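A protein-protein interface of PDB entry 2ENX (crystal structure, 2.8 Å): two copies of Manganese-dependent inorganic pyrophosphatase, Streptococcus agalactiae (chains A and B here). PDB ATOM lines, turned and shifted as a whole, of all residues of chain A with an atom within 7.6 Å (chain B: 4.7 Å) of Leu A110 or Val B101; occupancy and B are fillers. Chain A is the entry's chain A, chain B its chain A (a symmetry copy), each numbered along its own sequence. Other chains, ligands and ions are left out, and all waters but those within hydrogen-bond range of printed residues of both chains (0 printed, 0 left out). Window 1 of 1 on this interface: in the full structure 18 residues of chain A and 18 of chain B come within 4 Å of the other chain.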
ATOM      1  N   VAL A  72       8.378   5.951 -20.976  1.00  0.00           N
ATOM      2  CA  VAL A  72       9.459   6.144 -21.937  1.00  0.00           C
ATOM      3  C   VAL A  72       8.980   6.367 -23.374  1.00  0.00           C
ATOM      4  O   VAL A  72       7.815   6.131 -23.705  1.00  0.00           O
ATOM      5  CB  VAL A  72      10.445   4.942 -21.948  1.00  0.00           C
ATOM      6  CG1 VAL A  72      10.944   4.620 -20.547  1.00  0.00           C
ATOM      7  CG2 VAL A  72       9.817   3.714 -22.603  1.00  0.00           C
ATOM      8  N   LEU A  74      10.590   5.230 -27.185  1.00  0.00           N
ATOM      9  CA  LEU A  74      11.631   4.541 -27.950  1.00  0.00           C
ATOM     10  C   LEU A  74      11.750   5.113 -29.352  1.00  0.00           C
ATOM     11  O   LEU A  74      10.729   5.324 -30.030  1.00  0.00           O
ATOM     12  CB  LEU A  74      11.309   3.050 -28.060  1.00  0.00           C
ATOM     13  CG  LEU A  74      10.729   2.330 -26.845  1.00  0.00           C
ATOM     14  CD1 LEU A  74      10.514   0.885 -27.215  1.00  0.00           C
ATOM     15  CD2 LEU A  74      11.605   2.462 -25.603  1.00  0.00           C
ATOM     16  N   THR A  91       5.809   2.001 -18.859  1.00  0.00           N
ATOM     17  CA  THR A  91       4.838   2.237 -19.909  1.00  0.00           C
ATOM     18  C   THR A  91       5.560   2.818 -21.103  1.00  0.00           C
ATOM     19  O   THR A  91       6.326   3.778 -20.951  1.00  0.00           O
ATOM     20  CB  THR A  91       3.805   3.225 -19.436  1.00  0.00           C
ATOM     21  OG1 THR A  91       3.250   2.726 -18.221  1.00  0.00           O
ATOM     22  CG2 THR A  91       2.699   3.406 -20.490  1.00  0.00           C
ATOM     23  N   VAL A  92       5.334   2.225 -22.276  1.00  0.00           N
ATOM     24  CA  VAL A  92       5.810   2.800 -23.534  1.00  0.00           C
ATOM     25  C   VAL A  92       4.825   3.923 -23.901  1.00  0.00           C
ATOM     26  O   VAL A  92       3.644   3.668 -24.132  1.00  0.00           O
ATOM     27  CB  VAL A  92       5.915   1.720 -24.676  1.00  0.00           C
ATOM     28  CG1 VAL A  92       6.196   2.357 -26.004  1.00  0.00           C
ATOM     29  CG2 VAL A  92       6.989   0.700 -24.389  1.00  0.00           C
ATOM     30  N   TYR A  93       5.274   5.166 -23.928  1.00  0.00           N
ATOM     31  CA  TYR A  93       4.357   6.225 -24.316  1.00  0.00           C
ATOM     32  C   TYR A  93       4.171   6.229 -25.840  1.00  0.00           C
ATOM     33  O   TYR A  93       3.052   6.237 -26.355  1.00  0.00           O
ATOM     34  CB  TYR A  93       4.843   7.585 -23.804  1.00  0.00           C
ATOM     35  CG  TYR A  93       3.894   8.750 -24.034  1.00  0.00           C
ATOM     36  CD1 TYR A  93       3.123   9.264 -22.982  1.00  0.00           C
ATOM     37  CD2 TYR A  93       3.775   9.354 -25.299  1.00  0.00           C
ATOM     38  CE1 TYR A  93       2.235  10.357 -23.172  1.00  0.00           C
ATOM     39  CE2 TYR A  93       2.890  10.441 -25.514  1.00  0.00           C
ATOM     40  CZ  TYR A  93       2.119  10.944 -24.439  1.00  0.00           C
ATOM     41  OH  TYR A  93       1.252  12.027 -24.631  1.00  0.00           O
ATOM     42  N   GLY A  94       5.282   6.210 -26.556  1.00  0.00           N
ATOM     43  CA  GLY A  94       5.250   6.363 -27.988  1.00  0.00           C
ATOM     44  C   GLY A  94       6.469   5.718 -28.580  1.00  0.00           C
ATOM     45  O   GLY A  94       7.480   5.561 -27.889  1.00  0.00           O
ATOM     46  N   VAL A  95       6.357   5.323 -29.852  1.00  0.00           N
ATOM     47  CA  VAL A  95       7.477   4.752 -30.609  1.00  0.00           C
ATOM     48  C   VAL A  95       7.609   5.432 -31.972  1.00  0.00           C
ATOM     49  O   VAL A  95       6.637   5.565 -32.720  1.00  0.00           O
ATOM     50  CB  VAL A  95       7.340   3.214 -30.813  1.00  0.00           C
ATOM     51  CG1 VAL A  95       8.502   2.665 -31.646  1.00  0.00           C
ATOM     52  CG2 VAL A  95       7.282   2.494 -29.494  1.00  0.00           C
ATOM     53  N   VAL A 101       8.666  -5.341 -36.628  1.00  0.00           N
ATOM     54  CA  VAL A 101       8.160  -5.441 -35.252  1.00  0.00           C
ATOM     55  C   VAL A 101       8.173  -6.887 -34.724  1.00  0.00           C
ATOM     56  O   VAL A 101       7.676  -7.805 -35.387  1.00  0.00           O
ATOM     57  CB  VAL A 101       6.729  -4.844 -35.091  1.00  0.00           C
ATOM     58  CG1 VAL A 101       6.352  -4.755 -33.606  1.00  0.00           C
ATOM     59  CG2 VAL A 101       6.637  -3.487 -35.739  1.00  0.00           C
ATOM     60  N   PHE A 104       7.376  -7.170 -28.805  1.00  0.00           N
ATOM     61  CA  PHE A 104       6.904  -5.860 -28.360  1.00  0.00           C
ATOM     62  C   PHE A 104       5.412  -5.942 -28.000  1.00  0.00           C
ATOM     63  O   PHE A 104       4.595  -6.298 -28.850  1.00  0.00           O
ATOM     64  CB  PHE A 104       7.125  -4.836 -29.487  1.00  0.00           C
ATOM     65  CG  PHE A 104       6.538  -3.473 -29.213  1.00  0.00           C
ATOM     66  CD1 PHE A 104       5.369  -3.070 -29.838  1.00  0.00           C
ATOM     67  CD2 PHE A 104       7.169  -2.580 -28.338  1.00  0.00           C
ATOM     68  CE1 PHE A 104       4.822  -1.807 -29.590  1.00  0.00           C
ATOM     69  CE2 PHE A 104       6.627  -1.302 -28.077  1.00  0.00           C
ATOM     70  CZ  PHE A 104       5.456  -0.918 -28.705  1.00  0.00           C
ATOM     71  N   GLU A 105       5.065  -5.633 -26.749  1.00  0.00           N
ATOM     72  CA  GLU A 105       3.666  -5.615 -26.328  1.00  0.00           C
ATOM     73  C   GLU A 105       3.377  -4.555 -25.261  1.00  0.00           C
ATOM     74  O   GLU A 105       4.297  -4.055 -24.621  1.00  0.00           O
ATOM     75  CB  GLU A 105       3.182  -7.007 -25.904  1.00  0.00           C
ATOM     76  CG  GLU A 105       4.014  -7.691 -24.828  1.00  0.00           C
ATOM     77  CD  GLU A 105       3.426  -9.034 -24.346  1.00  0.00           C
ATOM     78  OE1 GLU A 105       3.480  -9.282 -23.128  1.00  0.00           O
ATOM     79  OE2 GLU A 105       2.918  -9.848 -25.162  1.00  0.00           O
ATOM     80  N   THR A 106       2.101  -4.190 -25.104  1.00  0.00           N
ATOM     81  CA  THR A 106       1.689  -3.117 -24.184  1.00  0.00           C
ATOM     82  C   THR A 106       0.342  -3.401 -23.501  1.00  0.00           C
ATOM     83  O   THR A 106      -0.350  -4.357 -23.842  1.00  0.00           O
ATOM     84  CB  THR A 106       1.625  -1.725 -24.888  1.00  0.00           C
ATOM     85  OG1 THR A 106       0.621  -1.742 -25.919  1.00  0.00           O
ATOM     86  CG2 THR A 106       2.991  -1.337 -25.487  1.00  0.00           C
ATOM     87  N   ALA A 107      -0.020  -2.578 -22.526  1.00  0.00           N
ATOM     88  CA  ALA A 107      -1.252  -2.794 -21.775  1.00  0.00           C
ATOM     89  C   ALA A 107      -2.347  -1.845 -22.257  1.00  0.00           C
ATOM     90  O   ALA A 107      -3.549  -2.100 -22.062  1.00  0.00           O
ATOM     91  CB  ALA A 107      -1.013  -2.634 -20.259  1.00  0.00           C
ATOM     92  N   ASN A 108      -1.911  -0.754 -22.890  1.00  0.00           N
ATOM     93  CA  ASN A 108      -2.780   0.356 -23.258  1.00  0.00           C
ATOM     94  C   ASN A 108      -2.413   0.888 -24.631  1.00  0.00           C
ATOM     95  O   ASN A 108      -1.343   0.556 -25.154  1.00  0.00           O
ATOM     96  CB  ASN A 108      -2.694   1.457 -22.212  1.00  0.00           C
ATOM     97  CG  ASN A 108      -2.982   0.940 -20.816  1.00  0.00           C
ATOM     98  OD1 ASN A 108      -4.139   0.841 -20.394  1.00  0.00           O
ATOM     99  ND2 ASN A 108      -1.924   0.580 -20.097  1.00  0.00           N
ATOM    100  N   PRO A 109      -3.313   1.684 -25.242  1.00  0.00           N
ATOM    101  CA  PRO A 109      -3.000   2.213 -26.585  1.00  0.00           C
ATOM    102  C   PRO A 109      -1.944   3.290 -26.534  1.00  0.00           C
ATOM    103  O   PRO A 109      -1.975   4.150 -25.657  1.00  0.00           O
ATOM    104  CB  PRO A 109      -4.335   2.777 -27.089  1.00  0.00           C
ATOM    105  CG  PRO A 109      -5.168   2.989 -25.843  1.00  0.00           C
ATOM    106  CD  PRO A 109      -4.647   2.088 -24.751  1.00  0.00           C
ATOM    107  N   LEU A 110      -1.012   3.238 -27.475  1.00  0.00           N
ATOM    108  CA  LEU A 110       0.085   4.183 -27.489  1.00  0.00           C
ATOM    109  C   LEU A 110       0.097   4.990 -28.752  1.00  0.00           C
ATOM    110  O   LEU A 110      -0.816   4.897 -29.551  1.00  0.00           O
ATOM    111  CB  LEU A 110       1.415   3.467 -27.296  1.00  0.00           C
ATOM    112  CG  LEU A 110       1.931   2.462 -28.316  1.00  0.00           C
ATOM    113  CD1 LEU A 110       3.351   2.140 -27.952  1.00  0.00           C
ATOM    114  CD2 LEU A 110       1.105   1.184 -28.374  1.00  0.00           C
ATOM    115  N   TYR A 111       1.114   5.824 -28.892  1.00  0.00           N
ATOM    116  CA  TYR A 111       1.394   6.494 -30.142  1.00  0.00           C
ATOM    117  C   TYR A 111       2.476   5.674 -30.790  1.00  0.00           C
ATOM    118  O   TYR A 111       3.470   5.330 -30.145  1.00  0.00           O
ATOM    119  CB  TYR A 111       1.972   7.878 -29.908  1.00  0.00           C
ATOM    120  CG  TYR A 111       1.021   8.954 -29.471  1.00  0.00           C
ATOM    121  CD1 TYR A 111       0.313   9.711 -30.416  1.00  0.00           C
ATOM    122  CD2 TYR A 111       0.863   9.266 -28.112  1.00  0.00           C
ATOM    123  CE1 TYR A 111      -0.554  10.759 -30.026  1.00  0.00           C
ATOM    124  CE2 TYR A 111      -0.016  10.309 -27.698  1.00  0.00           C
ATOM    125  CZ  TYR A 111      -0.717  11.049 -28.673  1.00  0.00           C
ATOM    126  OH  TYR A 111      -1.565  12.065 -28.295  1.00  0.00           O
ATOM    127  N   MET A 112       2.294   5.358 -32.064  1.00  0.00           N
ATOM    128  CA  MET A 112       3.363   4.774 -32.847  1.00  0.00           C
ATOM    129  C   MET A 112       3.390   5.523 -34.154  1.00  0.00           C
ATOM    130  O   MET A 112       2.380   6.072 -34.582  1.00  0.00           O
ATOM    131  CB  MET A 112       3.134   3.278 -33.065  1.00  0.00           C
ATOM    132  CG  MET A 112       3.124   2.419 -31.789  1.00  0.00           C
ATOM    133  SD  MET A 112       3.107   0.635 -32.099  1.00  0.00           S
ATOM    134  CE  MET A 112       4.805   0.310 -32.537  1.00  0.00           C
ATOM    135  N   ARG A 113       4.559   5.568 -34.770  1.00  0.00           N
ATOM    136  CA  ARG A 113       4.740   6.209 -36.052  1.00  0.00           C
ATOM    137  C   ARG A 113       5.906   5.482 -36.676  1.00  0.00           C
ATOM    138  O   ARG A 113       7.056   5.869 -36.506  1.00  0.00           O
ATOM    139  CB  ARG A 113       5.045   7.703 -35.865  1.00  0.00           C
ATOM    140  CG  ARG A 113       5.230   8.531 -37.167  1.00  0.00           C
ATOM    141  CD  ARG A 113       3.907   9.064 -37.729  1.00  0.00           C
ATOM    142  NE  ARG A 113       4.053   9.696 -39.039  1.00  0.00           N
ATOM    143  CZ  ARG A 113       4.126  11.015 -39.256  1.00  0.00           C
ATOM    144  NH1 ARG A 113       4.056  11.881 -38.254  1.00  0.00           N
ATOM    145  NH2 ARG A 113       4.256  11.483 -40.494  1.00  0.00           N
ATOM    146  N   ASN B  78      -4.797  -5.173 -34.451  1.00  0.00           N
ATOM    147  CA  ASN B  78      -3.438  -5.579 -34.809  1.00  0.00           C
ATOM    148  C   ASN B  78      -3.096  -6.948 -34.263  1.00  0.00           C
ATOM    149  O   ASN B  78      -2.136  -7.575 -34.708  1.00  0.00           O
ATOM    150  CB  ASN B  78      -2.408  -4.592 -34.278  1.00  0.00           C
ATOM    151  CG  ASN B  78      -2.348  -4.578 -32.770  1.00  0.00           C
ATOM    152  OD1 ASN B  78      -1.734  -5.442 -32.141  1.00  0.00           O
ATOM    153  ND2 ASN B  78      -2.986  -3.589 -32.177  1.00  0.00           N
ATOM    154  N   HIS B  99      -5.640   0.759 -30.440  1.00  0.00           N
ATOM    155  CA  HIS B  99      -5.605  -0.247 -29.360  1.00  0.00           C
ATOM    156  C   HIS B  99      -4.180  -0.508 -28.828  1.00  0.00           C
ATOM    157  O   HIS B  99      -3.181  -0.086 -29.428  1.00  0.00           O
ATOM    158  CB  HIS B  99      -6.185  -1.587 -29.844  1.00  0.00           C
ATOM    159  CG  HIS B  99      -7.647  -1.550 -30.157  1.00  0.00           C
ATOM    160  ND1 HIS B  99      -8.135  -1.155 -31.383  1.00  0.00           N
ATOM    161  CD2 HIS B  99      -8.726  -1.902 -29.419  1.00  0.00           C
ATOM    162  CE1 HIS B  99      -9.452  -1.247 -31.381  1.00  0.00           C
ATOM    163  NE2 HIS B  99      -9.835  -1.701 -30.202  1.00  0.00           N
ATOM    164  N   ARG B 100      -4.101  -1.207 -27.698  1.00  0.00           N
ATOM    165  CA  ARG B 100      -2.836  -1.742 -27.234  1.00  0.00           C
ATOM    166  C   ARG B 100      -2.270  -2.719 -28.292  1.00  0.00           C
ATOM    167  O   ARG B 100      -2.991  -3.144 -29.206  1.00  0.00           O
ATOM    168  CB  ARG B 100      -3.012  -2.397 -25.858  1.00  0.00           C
ATOM    169  CG  ARG B 100      -3.754  -3.719 -25.834  1.00  0.00           C
ATOM    170  CD  ARG B 100      -2.792  -4.856 -25.668  1.00  0.00           C
ATOM    171  NE  ARG B 100      -3.448  -6.148 -25.770  1.00  0.00           N
ATOM    172  CZ  ARG B 100      -3.788  -6.916 -24.735  1.00  0.00           C
ATOM    173  NH1 ARG B 100      -4.382  -8.079 -24.956  1.00  0.00           N
ATOM    174  NH2 ARG B 100      -3.542  -6.545 -23.478  1.00  0.00           N
ATOM    175  N   VAL B 101      -0.981  -3.039 -28.178  1.00  0.00           N
ATOM    176  CA  VAL B 101      -0.328  -3.975 -29.102  1.00  0.00           C
ATOM    177  C   VAL B 101       0.058  -5.301 -28.420  1.00  0.00           C
ATOM    178  O   VAL B 101       0.686  -5.303 -27.356  1.00  0.00           O
ATOM    179  CB  VAL B 101       0.930  -3.363 -29.790  1.00  0.00           C
ATOM    180  CG1 VAL B 101       1.428  -4.285 -30.912  1.00  0.00           C
ATOM    181  CG2 VAL B 101       0.632  -1.990 -30.333  1.00  0.00           C
ATOM    182  N   ALA B 102      -0.345  -6.408 -29.046  1.00  0.00           N
ATOM    183  CA  ALA B 102       0.035  -7.758 -28.632  1.00  0.00           C
ATOM    184  C   ALA B 102      -0.044  -8.733 -29.807  1.00  0.00           C
ATOM    185  O   ALA B 102      -0.644  -8.429 -30.831  1.00  0.00           O
ATOM    186  CB  ALA B 102      -0.849  -8.229 -27.500  1.00  0.00           C
ATOM    187  N   PHE B 104       1.506  -9.562 -32.357  1.00  0.00           N
ATOM    188  CA  PHE B 104       1.697  -8.916 -33.655  1.00  0.00           C
ATOM    189  C   PHE B 104       3.195  -8.875 -33.997  1.00  0.00           C
ATOM    190  O   PHE B 104       3.981  -8.302 -33.242  1.00  0.00           O
ATOM    191  CB  PHE B 104       1.125  -7.489 -33.598  1.00  0.00           C
ATOM    192  CG  PHE B 104       1.398  -6.660 -34.829  1.00  0.00           C
ATOM    193  CD1 PHE B 104       2.367  -5.670 -34.811  1.00  0.00           C
ATOM    194  CD2 PHE B 104       0.667  -6.857 -36.006  1.00  0.00           C
ATOM    195  CE1 PHE B 104       2.622  -4.896 -35.947  1.00  0.00           C
ATOM    196  CE2 PHE B 104       0.915  -6.085 -37.162  1.00  0.00           C
ATOM    197  CZ  PHE B 104       1.890  -5.104 -37.129  1.00  0.00           C
ATOM    198  N   LEU B 114      -0.414   4.547 -35.004  1.00  0.00           N
ATOM    199  CA  LEU B 114      -1.300   4.327 -33.879  1.00  0.00           C
ATOM    200  C   LEU B 114      -1.315   5.577 -33.009  1.00  0.00           C
ATOM    201  O   LEU B 114      -0.253   6.131 -32.685  1.00  0.00           O
ATOM    202  CB  LEU B 114      -0.849   3.107 -33.085  1.00  0.00           C
ATOM    203  CG  LEU B 114      -1.328   1.728 -33.557  1.00  0.00           C
ATOM    204  CD1 LEU B 114      -0.842   1.329 -34.943  1.00  0.00           C
ATOM    205  CD2 LEU B 114      -0.887   0.695 -32.559  1.00  0.00           C
ATOM    206  N   GLU B 115      -2.510   6.055 -32.676  1.00  0.00           N
ATOM    207  CA  GLU B 115      -2.666   7.138 -31.697  1.00  0.00           C
ATOM    208  C   GLU B 115      -3.759   6.710 -30.724  1.00  0.00           C
ATOM    209  O   GLU B 115      -4.701   6.006 -31.139  1.00  0.00           O
ATOM    210  CB  GLU B 115      -3.059   8.466 -32.356  1.00  0.00           C
ATOM    211  CG  GLU B 115      -2.360   8.793 -33.676  1.00  0.00           C
ATOM    212  CD  GLU B 115      -2.695  10.182 -34.216  1.00  0.00           C
ATOM    213  OE1 GLU B 115      -2.194  10.503 -35.317  1.00  0.00           O
ATOM    214  OE2 GLU B 115      -3.445  10.951 -33.552  1.00  0.00           O
ATOM    215  N   PRO B 116      -3.638   7.102 -29.434  1.00  0.00           N
ATOM    216  CA  PRO B 116      -4.631   6.746 -28.444  1.00  0.00           C
ATOM    217  C   PRO B 116      -5.751   7.775 -28.419  1.00  0.00           C
ATOM    218  O   PRO B 116      -5.680   8.771 -27.701  1.00  0.00           O
ATOM    219  CB  PRO B 116      -3.846   6.765 -27.141  1.00  0.00           C
ATOM    220  CG  PRO B 116      -2.655   7.604 -27.389  1.00  0.00           C
ATOM    221  CD  PRO B 116      -2.548   7.893 -28.844  1.00  0.00           C
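Leu A110 touches just these residues of chain B: Val B101 (3.8 Å), Leu B114 (3.4 Å), Glu B115 (3.6 Å) and Pro B116 (3.5 Å). Printed residues of chain A within 4 Å of Val B101: Glu A105 (3.2 Å), Thr A106 (2.9 Å) and Leu A110 (3.8 Å). Printed residues of chain B within 4 Å of Thr A106: Arg B100 and Val B101. Printed residues of chain A within 4 Å of Leu B114: Leu A110 (3.4 Å), Tyr A111 (3.1 Å) and Met A112 (2.7 Å). Of the printed residues of chain B, Pro A109 touches His B99, Arg B100 and Pro B116. Printed residues of chain A within 4 Å of Glu B115: Leu A110 (3.6 Å). The nearest printed residue of chain B that does not touch Pro A109 is Glu B115 (5.2 Å).
The backbone NH (N) of Thr A106 is in hydrogen-bond range of the backbone carbonyl oxygen (O) of Val B101 (2.9 Å). O of Leu B114 is in hydrogen-bond range of N of Met A112 (2.7 Å). O of Leu A110 lies close to O of Leu B114 (3.4 Å).
Positions printed for both chains: 101 and 104.
Among the printed residues, merely in contact across the chains: Glu A105 with Val B101 (3.2 Å), Thr A106 with Arg B100 (3.1 Å), Ala A107 with Arg B100 (3.7 Å), Asn A108 with Arg B100 (3.4 Å), Pro A109 with His B99 (3.7 Å), Pro A109 with Arg B100 (3.8 Å), Pro A109 with Pro B116 (3.5 Å), Leu A110 with Val B101 (3.8 Å), Leu A110 with Glu B115 (3.6 Å), Leu A110 with Pro B116 (3.5 Å), Tyr A111 with Leu B114 (3.1 Å) and Tyr A111 with Pro B116 (3.7 Å).
Of the 9 printed residues of chain B, 6 touch a printed residue of chain A. Hydrophobic or aromatic side chains of chain B that line the printed part of chain A: Val B101, Leu B114 and Pro B116. Along chain B the printed residues that touch a printed residue of chain A span positions 99 to 116. Of the 18 printed residues of chain A, 8 touch a printed residue of chain B. Hydrophobic or aromatic side chains of chain A that line the printed part of chain B: Pro A109, Leu A110, Tyr A111 and Met A112.
The backbone carbonyl oxygen (O) of Tyr A93 is in hydrogen-bond range of the backbone NH (N) of Tyr A111. O of Tyr A111 lies within hydrogen-bond range of N of Val A95, 2.9 Å away. OG1 of Thr A106 sits at hydrogen-bond distance from O of Asn A108 (3.1 Å). The side-chain amide nitrogen (ND2) of Asn B78 sits at hydrogen-bond distance from the backbone carbonyl oxygen (O) of Arg B100 (3.0 Å).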
